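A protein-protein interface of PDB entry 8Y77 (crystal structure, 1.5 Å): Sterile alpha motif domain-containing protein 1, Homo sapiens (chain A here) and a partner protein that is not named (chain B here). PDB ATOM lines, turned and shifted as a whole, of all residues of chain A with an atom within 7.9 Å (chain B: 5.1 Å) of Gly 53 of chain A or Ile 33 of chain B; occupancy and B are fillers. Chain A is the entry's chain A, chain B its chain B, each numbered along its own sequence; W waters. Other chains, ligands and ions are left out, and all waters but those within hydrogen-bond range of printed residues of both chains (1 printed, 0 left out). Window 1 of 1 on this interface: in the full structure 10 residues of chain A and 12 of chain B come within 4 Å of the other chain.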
ATOM      1  N   PHE A  19      16.628   0.257  23.155  1.00  0.00           N
ATOM      2  CA  PHE A  19      17.743   0.924  23.826  1.00  0.00           C
ATOM      3  C   PHE A  19      17.418   1.116  25.307  1.00  0.00           C
ATOM      4  O   PHE A  19      17.493   2.238  25.823  1.00  0.00           O
ATOM      5  CB  PHE A  19      18.045   2.268  23.164  1.00  0.00           C
ATOM      6  CG  PHE A  19      18.394   2.165  21.704  1.00  0.00           C
ATOM      7  CD1 PHE A  19      19.688   1.890  21.302  1.00  0.00           C
ATOM      8  CD2 PHE A  19      17.426   2.377  20.738  1.00  0.00           C
ATOM      9  CE1 PHE A  19      20.007   1.806  19.952  1.00  0.00           C
ATOM     10  CE2 PHE A  19      17.738   2.293  19.385  1.00  0.00           C
ATOM     11  CZ  PHE A  19      19.032   2.011  18.995  1.00  0.00           C
ATOM     12  N   GLN A  22      20.290   2.674  27.421  1.00  0.00           N
ATOM     13  CA  GLN A  22      20.558   4.067  27.091  1.00  0.00           C
ATOM     14  C   GLN A  22      19.410   4.970  27.520  1.00  0.00           C
ATOM     15  O   GLN A  22      19.621   6.158  27.789  1.00  0.00           O
ATOM     16  CB  GLN A  22      20.819   4.199  25.589  1.00  0.00           C
ATOM     17  CG  GLN A  22      22.114   3.545  25.122  1.00  0.00           C
ATOM     18  CD  GLN A  22      21.986   2.043  24.966  1.00  0.00           C
ATOM     19  OE1 GLN A  22      20.928   1.536  24.613  1.00  0.00           O
ATOM     20  NE2 GLN A  22      23.067   1.324  25.234  1.00  0.00           N
ATOM     21  N   LEU A  45      26.527  11.827  21.173  1.00  0.00           N
ATOM     22  CA  LEU A  45      27.666  10.917  21.185  1.00  0.00           C
ATOM     23  C   LEU A  45      28.546  11.090  22.420  1.00  0.00           C
ATOM     24  O   LEU A  45      29.197  10.126  22.845  1.00  0.00           O
ATOM     25  CB  LEU A  45      28.503  11.097  19.911  1.00  0.00           C
ATOM     26  CG  LEU A  45      27.789  10.972  18.559  1.00  0.00           C
ATOM     27  CD1 LEU A  45      28.800  11.000  17.395  1.00  0.00           C
ATOM     28  CD2 LEU A  45      26.915   9.742  18.485  1.00  0.00           C
ATOM     29  N   ILE A  50      26.732   7.154  27.308  1.00  0.00           N
ATOM     30  CA  ILE A  50      26.305   5.910  26.686  1.00  0.00           C
ATOM     31  C   ILE A  50      27.373   5.470  25.693  1.00  0.00           C
ATOM     32  O   ILE A  50      28.242   6.246  25.298  1.00  0.00           O
ATOM     33  CB  ILE A  50      24.921   6.016  26.016  1.00  0.00           C
ATOM     34  CG1 ILE A  50      24.945   7.042  24.879  1.00  0.00           C
ATOM     35  CG2 ILE A  50      23.850   6.369  27.063  1.00  0.00           C
ATOM     36  CD1 ILE A  50      23.638   7.106  24.110  1.00  0.00           C
ATOM     37  N   ARG A  51      27.313   4.198  25.312  1.00  0.00           N
ATOM     38  CA  ARG A  51      28.284   3.669  24.361  1.00  0.00           C
ATOM     39  C   ARG A  51      28.061   4.262  22.970  1.00  0.00           C
ATOM     40  O   ARG A  51      26.937   4.578  22.573  1.00  0.00           O
ATOM     41  CB  ARG A  51      28.182   2.145  24.290  1.00  0.00           C
ATOM     42  CG  ARG A  51      28.571   1.415  25.575  1.00  0.00           C
ATOM     43  CD  ARG A  51      29.950   1.815  26.063  1.00  0.00           C
ATOM     44  NE  ARG A  51      30.382   0.976  27.177  1.00  0.00           N
ATOM     45  CZ  ARG A  51      31.654   0.735  27.485  1.00  0.00           C
ATOM     46  NH1 ARG A  51      32.628   1.270  26.760  1.00  0.00           N
ATOM     47  NH2 ARG A  51      31.950  -0.041  28.521  1.00  0.00           N
ATOM     48  N   LEU A  52      29.151   4.364  22.207  1.00  0.00           N
ATOM     49  CA  LEU A  52      29.115   5.121  20.955  1.00  0.00           C
ATOM     50  C   LEU A  52      28.245   4.440  19.904  1.00  0.00           C
ATOM     51  O   LEU A  52      27.554   5.118  19.138  1.00  0.00           O
ATOM     52  CB  LEU A  52      30.536   5.296  20.430  1.00  0.00           C
ATOM     53  CG  LEU A  52      30.715   6.240  19.256  1.00  0.00           C
ATOM     54  CD1 LEU A  52      30.074   7.588  19.561  1.00  0.00           C
ATOM     55  CD2 LEU A  52      32.202   6.386  18.964  1.00  0.00           C
ATOM     56  N   GLY A  53      28.268   3.109  19.837  1.00  0.00           N
ATOM     57  CA  GLY A  53      27.478   2.393  18.862  1.00  0.00           C
ATOM     58  C   GLY A  53      25.994   2.684  18.970  1.00  0.00           C
ATOM     59  O   GLY A  53      25.353   3.157  18.020  1.00  0.00           O
ATOM     60  N   PRO A  54      25.425   2.425  20.146  1.00  0.00           N
ATOM     61  CA  PRO A  54      24.034   2.830  20.389  1.00  0.00           C
ATOM     62  C   PRO A  54      23.805   4.311  20.164  1.00  0.00           C
ATOM     63  O   PRO A  54      22.768   4.694  19.609  1.00  0.00           O
ATOM     64  CB  PRO A  54      23.812   2.446  21.859  1.00  0.00           C
ATOM     65  CG  PRO A  54      24.806   1.349  22.114  1.00  0.00           C
ATOM     66  CD  PRO A  54      25.997   1.652  21.263  1.00  0.00           C
ATOM     67  N   ALA A  55      24.748   5.154  20.586  1.00  0.00           N
ATOM     68  CA  ALA A  55      24.554   6.597  20.457  1.00  0.00           C
ATOM     69  C   ALA A  55      24.411   7.015  19.002  1.00  0.00           C
ATOM     70  O   ALA A  55      23.559   7.849  18.669  1.00  0.00           O
ATOM     71  CB  ALA A  55      25.700   7.347  21.133  1.00  0.00           C
ATOM     72  N   LEU A  56      25.243   6.450  18.122  1.00  0.00           N
ATOM     73  CA  LEU A  56      25.153   6.747  16.695  1.00  0.00           C
ATOM     74  C   LEU A  56      23.783   6.379  16.146  1.00  0.00           C
ATOM     75  O   LEU A  56      23.201   7.128  15.353  1.00  0.00           O
ATOM     76  CB  LEU A  56      26.236   5.967  15.939  1.00  0.00           C
ATOM     77  CG  LEU A  56      27.667   6.459  16.112  1.00  0.00           C
ATOM     78  CD1 LEU A  56      28.645   5.323  15.803  1.00  0.00           C
ATOM     79  CD2 LEU A  56      27.919   7.674  15.207  1.00  0.00           C
ATOM     80  N   LYS A  57      23.270   5.204  16.519  1.00  0.00           N
ATOM     81  CA  LYS A  57      21.957   4.796  16.031  1.00  0.00           C
ATOM     82  C   LYS A  57      20.861   5.671  16.621  1.00  0.00           C
ATOM     83  O   LYS A  57      19.898   6.031  15.924  1.00  0.00           O
ATOM     84  CB  LYS A  57      21.695   3.329  16.379  1.00  0.00           C
ATOM     85  CG  LYS A  57      22.726   2.345  15.836  1.00  0.00           C
ATOM     86  CD  LYS A  57      22.522   0.978  16.480  1.00  0.00           C
ATOM     87  CE  LYS A  57      23.226  -0.137  15.719  1.00  0.00           C
ATOM     88  NZ  LYS A  57      23.396  -1.334  16.601  1.00  0.00           N
ATOM     89  N   ILE A  58      20.973   5.994  17.913  1.00  0.00           N
ATOM     90  CA  ILE A  58      19.999   6.874  18.556  1.00  0.00           C
ATOM     91  C   ILE A  58      19.900   8.204  17.822  1.00  0.00           C
ATOM     92  O   ILE A  58      18.795   8.707  17.588  1.00  0.00           O
ATOM     93  CB  ILE A  58      20.326   7.041  20.051  1.00  0.00           C
ATOM     94  CG1 ILE A  58      19.912   5.772  20.796  1.00  0.00           C
ATOM     95  CG2 ILE A  58      19.593   8.248  20.640  1.00  0.00           C
ATOM     96  CD1 ILE A  58      20.484   5.684  22.202  1.00  0.00           C
ATOM     97  N   TYR A  59      21.038   8.790  17.437  1.00  0.00           N
ATOM     98  CA  TYR A  59      20.981  10.070  16.736  1.00  0.00           C
ATOM     99  C   TYR A  59      20.470   9.907  15.310  1.00  0.00           C
ATOM    100  O   TYR A  59      19.509  10.568  14.901  1.00  0.00           O
ATOM    101  CB  TYR A  59      22.337  10.788  16.721  1.00  0.00           C
ATOM    102  CG  TYR A  59      22.217  12.083  15.948  1.00  0.00           C
ATOM    103  CD1 TYR A  59      21.579  13.177  16.511  1.00  0.00           C
ATOM    104  CD2 TYR A  59      22.660  12.180  14.637  1.00  0.00           C
ATOM    105  CE1 TYR A  59      21.427  14.358  15.802  1.00  0.00           C
ATOM    106  CE2 TYR A  59      22.506  13.353  13.919  1.00  0.00           C
ATOM    107  CZ  TYR A  59      21.890  14.437  14.512  1.00  0.00           C
ATOM    108  OH  TYR A  59      21.732  15.612  13.811  1.00  0.00           O
ATOM    109  N   SER B   7      28.560  -8.293  13.035  1.00  0.00           N
ATOM    110  CA  SER B   7      28.548  -8.124  14.477  1.00  0.00           C
ATOM    111  C   SER B   7      29.625  -7.130  14.910  1.00  0.00           C
ATOM    112  O   SER B   7      30.537  -6.772  14.155  1.00  0.00           O
ATOM    113  CB  SER B   7      28.814  -9.457  15.174  1.00  0.00           C
ATOM    114  OG  SER B   7      30.119  -9.931  14.840  1.00  0.00           O
ATOM    115  N   THR B   8      29.519  -6.716  16.175  1.00  0.00           N
ATOM    116  CA  THR B   8      30.562  -5.907  16.793  1.00  0.00           C
ATOM    117  C   THR B   8      31.924  -6.587  16.696  1.00  0.00           C
ATOM    118  O   THR B   8      32.934  -5.938  16.392  1.00  0.00           O
ATOM    119  CB  THR B   8      30.178  -5.618  18.246  1.00  0.00           C
ATOM    120  OG1 THR B   8      28.984  -4.820  18.284  1.00  0.00           O
ATOM    121  CG2 THR B   8      31.276  -4.875  18.962  1.00  0.00           C
ATOM    122  N   VAL B  11      33.425  -6.200  13.199  1.00  0.00           N
ATOM    123  CA  VAL B  11      33.963  -4.866  12.941  1.00  0.00           C
ATOM    124  C   VAL B  11      35.330  -4.726  13.598  1.00  0.00           C
ATOM    125  O   VAL B  11      36.297  -4.256  12.980  1.00  0.00           O
ATOM    126  CB  VAL B  11      32.979  -3.793  13.441  1.00  0.00           C
ATOM    127  CG1 VAL B  11      33.619  -2.401  13.382  1.00  0.00           C
ATOM    128  CG2 VAL B  11      31.696  -3.821  12.605  1.00  0.00           C
ATOM    129  N   PHE B  28      36.459  -0.234  19.542  1.00  0.00           N
ATOM    130  CA  PHE B  28      35.247  -0.428  18.752  1.00  0.00           C
ATOM    131  C   PHE B  28      34.363  -1.502  19.370  1.00  0.00           C
ATOM    132  O   PHE B  28      33.135  -1.351  19.424  1.00  0.00           O
ATOM    133  CB  PHE B  28      35.594  -0.759  17.299  1.00  0.00           C
ATOM    134  CG  PHE B  28      35.952   0.452  16.481  1.00  0.00           C
ATOM    135  CD1 PHE B  28      37.220   1.015  16.571  1.00  0.00           C
ATOM    136  CD2 PHE B  28      35.028   1.024  15.633  1.00  0.00           C
ATOM    137  CE1 PHE B  28      37.551   2.149  15.824  1.00  0.00           C
ATOM    138  CE2 PHE B  28      35.348   2.148  14.882  1.00  0.00           C
ATOM    139  CZ  PHE B  28      36.607   2.716  14.981  1.00  0.00           C
ATOM    140  N   LYS B  29      34.973  -2.571  19.879  1.00  0.00           N
ATOM    141  CA  LYS B  29      34.206  -3.625  20.535  1.00  0.00           C
ATOM    142  C   LYS B  29      33.541  -3.108  21.803  1.00  0.00           C
ATOM    143  O   LYS B  29      32.351  -3.356  22.041  1.00  0.00           O
ATOM    144  CB  LYS B  29      35.112  -4.817  20.848  1.00  0.00           C
ATOM    145  CG  LYS B  29      34.559  -5.756  21.889  1.00  0.00           C
ATOM    146  CD  LYS B  29      33.487  -6.632  21.297  1.00  0.00           C
ATOM    147  CE  LYS B  29      34.090  -7.579  20.287  1.00  0.00           C
ATOM    148  NZ  LYS B  29      33.323  -8.845  20.220  1.00  0.00           N
ATOM    149  N   GLU B  31      32.670  -0.154  22.571  1.00  0.00           N
ATOM    150  CA  GLU B  31      31.624   0.810  22.259  1.00  0.00           C
ATOM    151  C   GLU B  31      30.447   0.177  21.532  1.00  0.00           C
ATOM    152  O   GLU B  31      29.523   0.892  21.132  1.00  0.00           O
ATOM    153  CB  GLU B  31      32.201   1.976  21.454  1.00  0.00           C
ATOM    154  CG  GLU B  31      33.214   2.800  22.230  1.00  0.00           C
ATOM    155  CD  GLU B  31      32.656   3.297  23.559  1.00  0.00           C
ATOM    156  OE1 GLU B  31      31.526   3.830  23.580  1.00  0.00           O
ATOM    157  OE2 GLU B  31      33.340   3.143  24.595  1.00  0.00           O
ATOM    158  N   GLN B  32      30.461  -1.143  21.361  1.00  0.00           N
ATOM    159  CA  GLN B  32      29.399  -1.873  20.669  1.00  0.00           C
ATOM    160  C   GLN B  32      29.146  -1.306  19.275  1.00  0.00           C
ATOM    161  O   GLN B  32      28.006  -1.093  18.855  1.00  0.00           O
ATOM    162  CB  GLN B  32      28.114  -1.934  21.501  1.00  0.00           C
ATOM    163  CG  GLN B  32      28.257  -2.776  22.755  1.00  0.00           C
ATOM    164  CD  GLN B  32      27.004  -2.771  23.618  1.00  0.00           C
ATOM    165  OE1 GLN B  32      25.956  -2.266  23.215  1.00  0.00           O
ATOM    166  NE2 GLN B  32      27.118  -3.323  24.820  1.00  0.00           N
ATOM    167  N   ILE B  33      30.227  -1.069  18.535  1.00  0.00           N
ATOM    168  CA  ILE B  33      30.099  -0.612  17.153  1.00  0.00           C
ATOM    169  C   ILE B  33      29.969  -1.861  16.282  1.00  0.00           C
ATOM    170  O   ILE B  33      30.957  -2.492  15.890  1.00  0.00           O
ATOM    171  CB  ILE B  33      31.233   0.326  16.748  1.00  0.00           C
ATOM    172  CG1 ILE B  33      31.132   1.613  17.582  1.00  0.00           C
ATOM    173  CG2 ILE B  33      31.151   0.645  15.266  1.00  0.00           C
ATOM    174  CD1 ILE B  33      32.346   2.517  17.477  1.00  0.00           C
ATOM    175  N   ASP B  34      28.720  -2.245  16.007  1.00  0.00           N
ATOM    176  CA  ASP B  34      28.450  -3.295  15.032  1.00  0.00           C
ATOM    177  C   ASP B  34      28.470  -2.699  13.627  1.00  0.00           C
ATOM    178  O   ASP B  34      28.753  -1.517  13.441  1.00  0.00           O
ATOM    179  CB  ASP B  34      27.140  -4.024  15.344  1.00  0.00           C
ATOM    180  CG  ASP B  34      25.917  -3.117  15.320  1.00  0.00           C
ATOM    181  OD1 ASP B  34      26.012  -1.932  14.937  1.00  0.00           O
ATOM    182  OD2 ASP B  34      24.825  -3.601  15.706  1.00  0.00           O
ATOM    183  N   GLY B  35      28.152  -3.516  12.625  1.00  0.00           N
ATOM    184  CA  GLY B  35      28.260  -3.042  11.252  1.00  0.00           C
ATOM    185  C   GLY B  35      27.328  -1.877  10.977  1.00  0.00           C
ATOM    186  O   GLY B  35      27.698  -0.914  10.302  1.00  0.00           O
ATOM    187  N   ALA B  37      26.228   0.428  13.080  1.00  0.00           N
ATOM    188  CA  ALA B  37      26.781   1.646  13.669  1.00  0.00           C
ATOM    189  C   ALA B  37      28.051   2.092  12.945  1.00  0.00           C
ATOM    190  O   ALA B  37      28.278   3.296  12.771  1.00  0.00           O
ATOM    191  CB  ALA B  37      27.072   1.417  15.152  1.00  0.00           C
ATOM    192  N   PHE B  38      28.891   1.139  12.526  1.00  0.00           N
ATOM    193  CA  PHE B  38      30.132   1.457  11.819  1.00  0.00           C
ATOM    194  C   PHE B  38      29.864   2.330  10.600  1.00  0.00           C
ATOM    195  O   PHE B  38      30.596   3.291  10.342  1.00  0.00           O
ATOM    196  CB  PHE B  38      30.788   0.136  11.391  1.00  0.00           C
ATOM    197  CG  PHE B  38      32.240   0.240  10.963  1.00  0.00           C
ATOM    198  CD1 PHE B  38      33.149   1.027  11.655  1.00  0.00           C
ATOM    199  CD2 PHE B  38      32.690  -0.520   9.901  1.00  0.00           C
ATOM    200  CE1 PHE B  38      34.477   1.065  11.268  1.00  0.00           C
ATOM    201  CE2 PHE B  38      34.018  -0.482   9.504  1.00  0.00           C
ATOM    202  CZ  PHE B  38      34.909   0.306  10.195  1.00  0.00           C
ATOM    203  N   MET B  41      29.700   6.239  10.999  1.00  0.00           N
ATOM    204  CA  MET B  41      30.818   6.971  11.581  1.00  0.00           C
ATOM    205  C   MET B  41      31.568   7.795  10.544  1.00  0.00           C
ATOM    206  O   MET B  41      31.570   7.479   9.355  1.00  0.00           O
ATOM    207  CB  MET B  41      31.790   5.987  12.229  1.00  0.00           C
ATOM    208  CG  MET B  41      31.148   5.229  13.337  1.00  0.00           C
ATOM    209  SD  MET B  41      32.294   4.240  14.277  1.00  0.00           S
ATOM    210  CE  MET B  41      33.273   5.501  15.086  1.00  0.00           C
ATOM    211  N   MET B  50      36.993   8.984  19.601  1.00  0.00           N
ATOM    212  CA  MET B  50      37.712   7.777  19.978  1.00  0.00           C
ATOM    213  C   MET B  50      39.195   8.007  20.222  1.00  0.00           C
ATOM    214  O   MET B  50      39.879   7.080  20.665  1.00  0.00           O
ATOM    215  CB  MET B  50      37.506   6.702  18.922  1.00  0.00           C
ATOM    216  CG  MET B  50      36.036   6.386  18.769  1.00  0.00           C
ATOM    217  SD  MET B  50      35.796   5.155  17.502  1.00  0.00           S
ATOM    218  CE  MET B  50      35.584   3.674  18.497  1.00  0.00           C
HETATM  219  O   HOH W   1      25.196  -0.997  18.981  1.00  0.00           O
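The guanidinium group of Arg 51 of chain A is in salt-bridge range of the side-chain carboxylate of Glu 31 of chain B (2.9 Å).
The side-chain carboxylate (OE1) of Glu 31 of chain B is in hydrogen-bond range of the backbone NH (N) of Leu 52 of chain A.
The side-chain carboxylate (OD2) of Asp 34 of chain B is in salt-bridge range of the side-chain amino group (NZ) of Lys 57 of chain A (2.8 Å).
The backbone NH (N) of Gly 53 of chain A sits at hydrogen-bond distance from the backbone carbonyl oxygen (O) of Glu 31 of chain B, 2.9 Å away.
N of Ala 37 of chain B is in hydrogen-bond range of OD1 of Asp 34 of chain B (3.0 Å).
The backbone carbonyl oxygen of Phe 28 of chain B lies within hydrogen-bond range of the backbone NH of Ile 33 of chain B, 3.1 Å away.
N of Asp 34 of chain B lies within hydrogen-bond range of OG1 of Thr 8 of chain B (3.4 Å).
Among the printed residues, pairs that only touch across the chains: Leu 52 of chain A with Met 50 of chain B (3.8 Å), Gly 53 of chain A with Gln 32 of chain B (3.5 Å), Gly 53 of chain A with Ile 33 of chain B (3.9 Å), Gly 53 of chain A with Ala 37 of chain B (3.8 Å), Pro 54 of chain A with Glu 31 of chain B (3.6 Å), Pro 54 of chain A with Gln 32 of chain B (3.95 Å), Leu 56 of chain A with Ala 37 of chain B (3.7 Å) and Leu 56 of chain A with Met 41 of chain B (3.5 Å).
Of chain B, only Glu 31 (2.9 Å), Gln 32 (3.5 Å), Ile 33 (3.9 Å) and Ala 37 (3.8 Å) come within 4 Å of Gly 53 of chain A.
Ala 55 of chain A touches none of the printed residues of chain B.
Of the printed residues of chain B, Leu 56 of chain A touches Ala 37 and Met 41.
Of the printed residues of chain B, Lys 57 of chain A touches Asp 34 (2.8 Å).
Of the printed residues of chain A, Glu 31 of chain B touches Arg 51 (2.9 Å), Leu 52 (2.8 Å), Gly 53 (2.9 Å) and Pro 54 (3.6 Å).
Ile 33 of chain B touches just one residue of chain A: Gly 53 (3.9 Å).
The nearest residue of chain A that does not touch Ile 33 of chain B is Leu 52 of chain A (4.1 Å).
Of the 14 printed residues of chain B, 7 touch a printed residue of chain A.
Hydrophobic or aromatic side chains of chain B that line the printed part of chain A: Ile 33, Ala 37, Met 41 and Met 50.
Of the 13 printed residues of chain A, 6 touch a printed residue of chain B.
Hydrophobic or aromatic side chains of chain A within 4 Å of the printed part of chain B: Leu 52, Pro 54 and Leu 56.
Among the printed residues, Asp or Glu carboxylates within 4 Å of a Lys or Arg side-chain nitrogen of the other chain: Arg 51 of chain A with Glu 31 of chain B (2.9 Å) and Lys 57 of chain A with Asp 34 of chain B (2.8 Å).
Water W1 bridges the backbone carbonyl oxygen (O) of Gln 32 of chain B (2.8 Å) and the side-chain amino group (NZ) of Lys 57 of chain A (3.0 Å).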
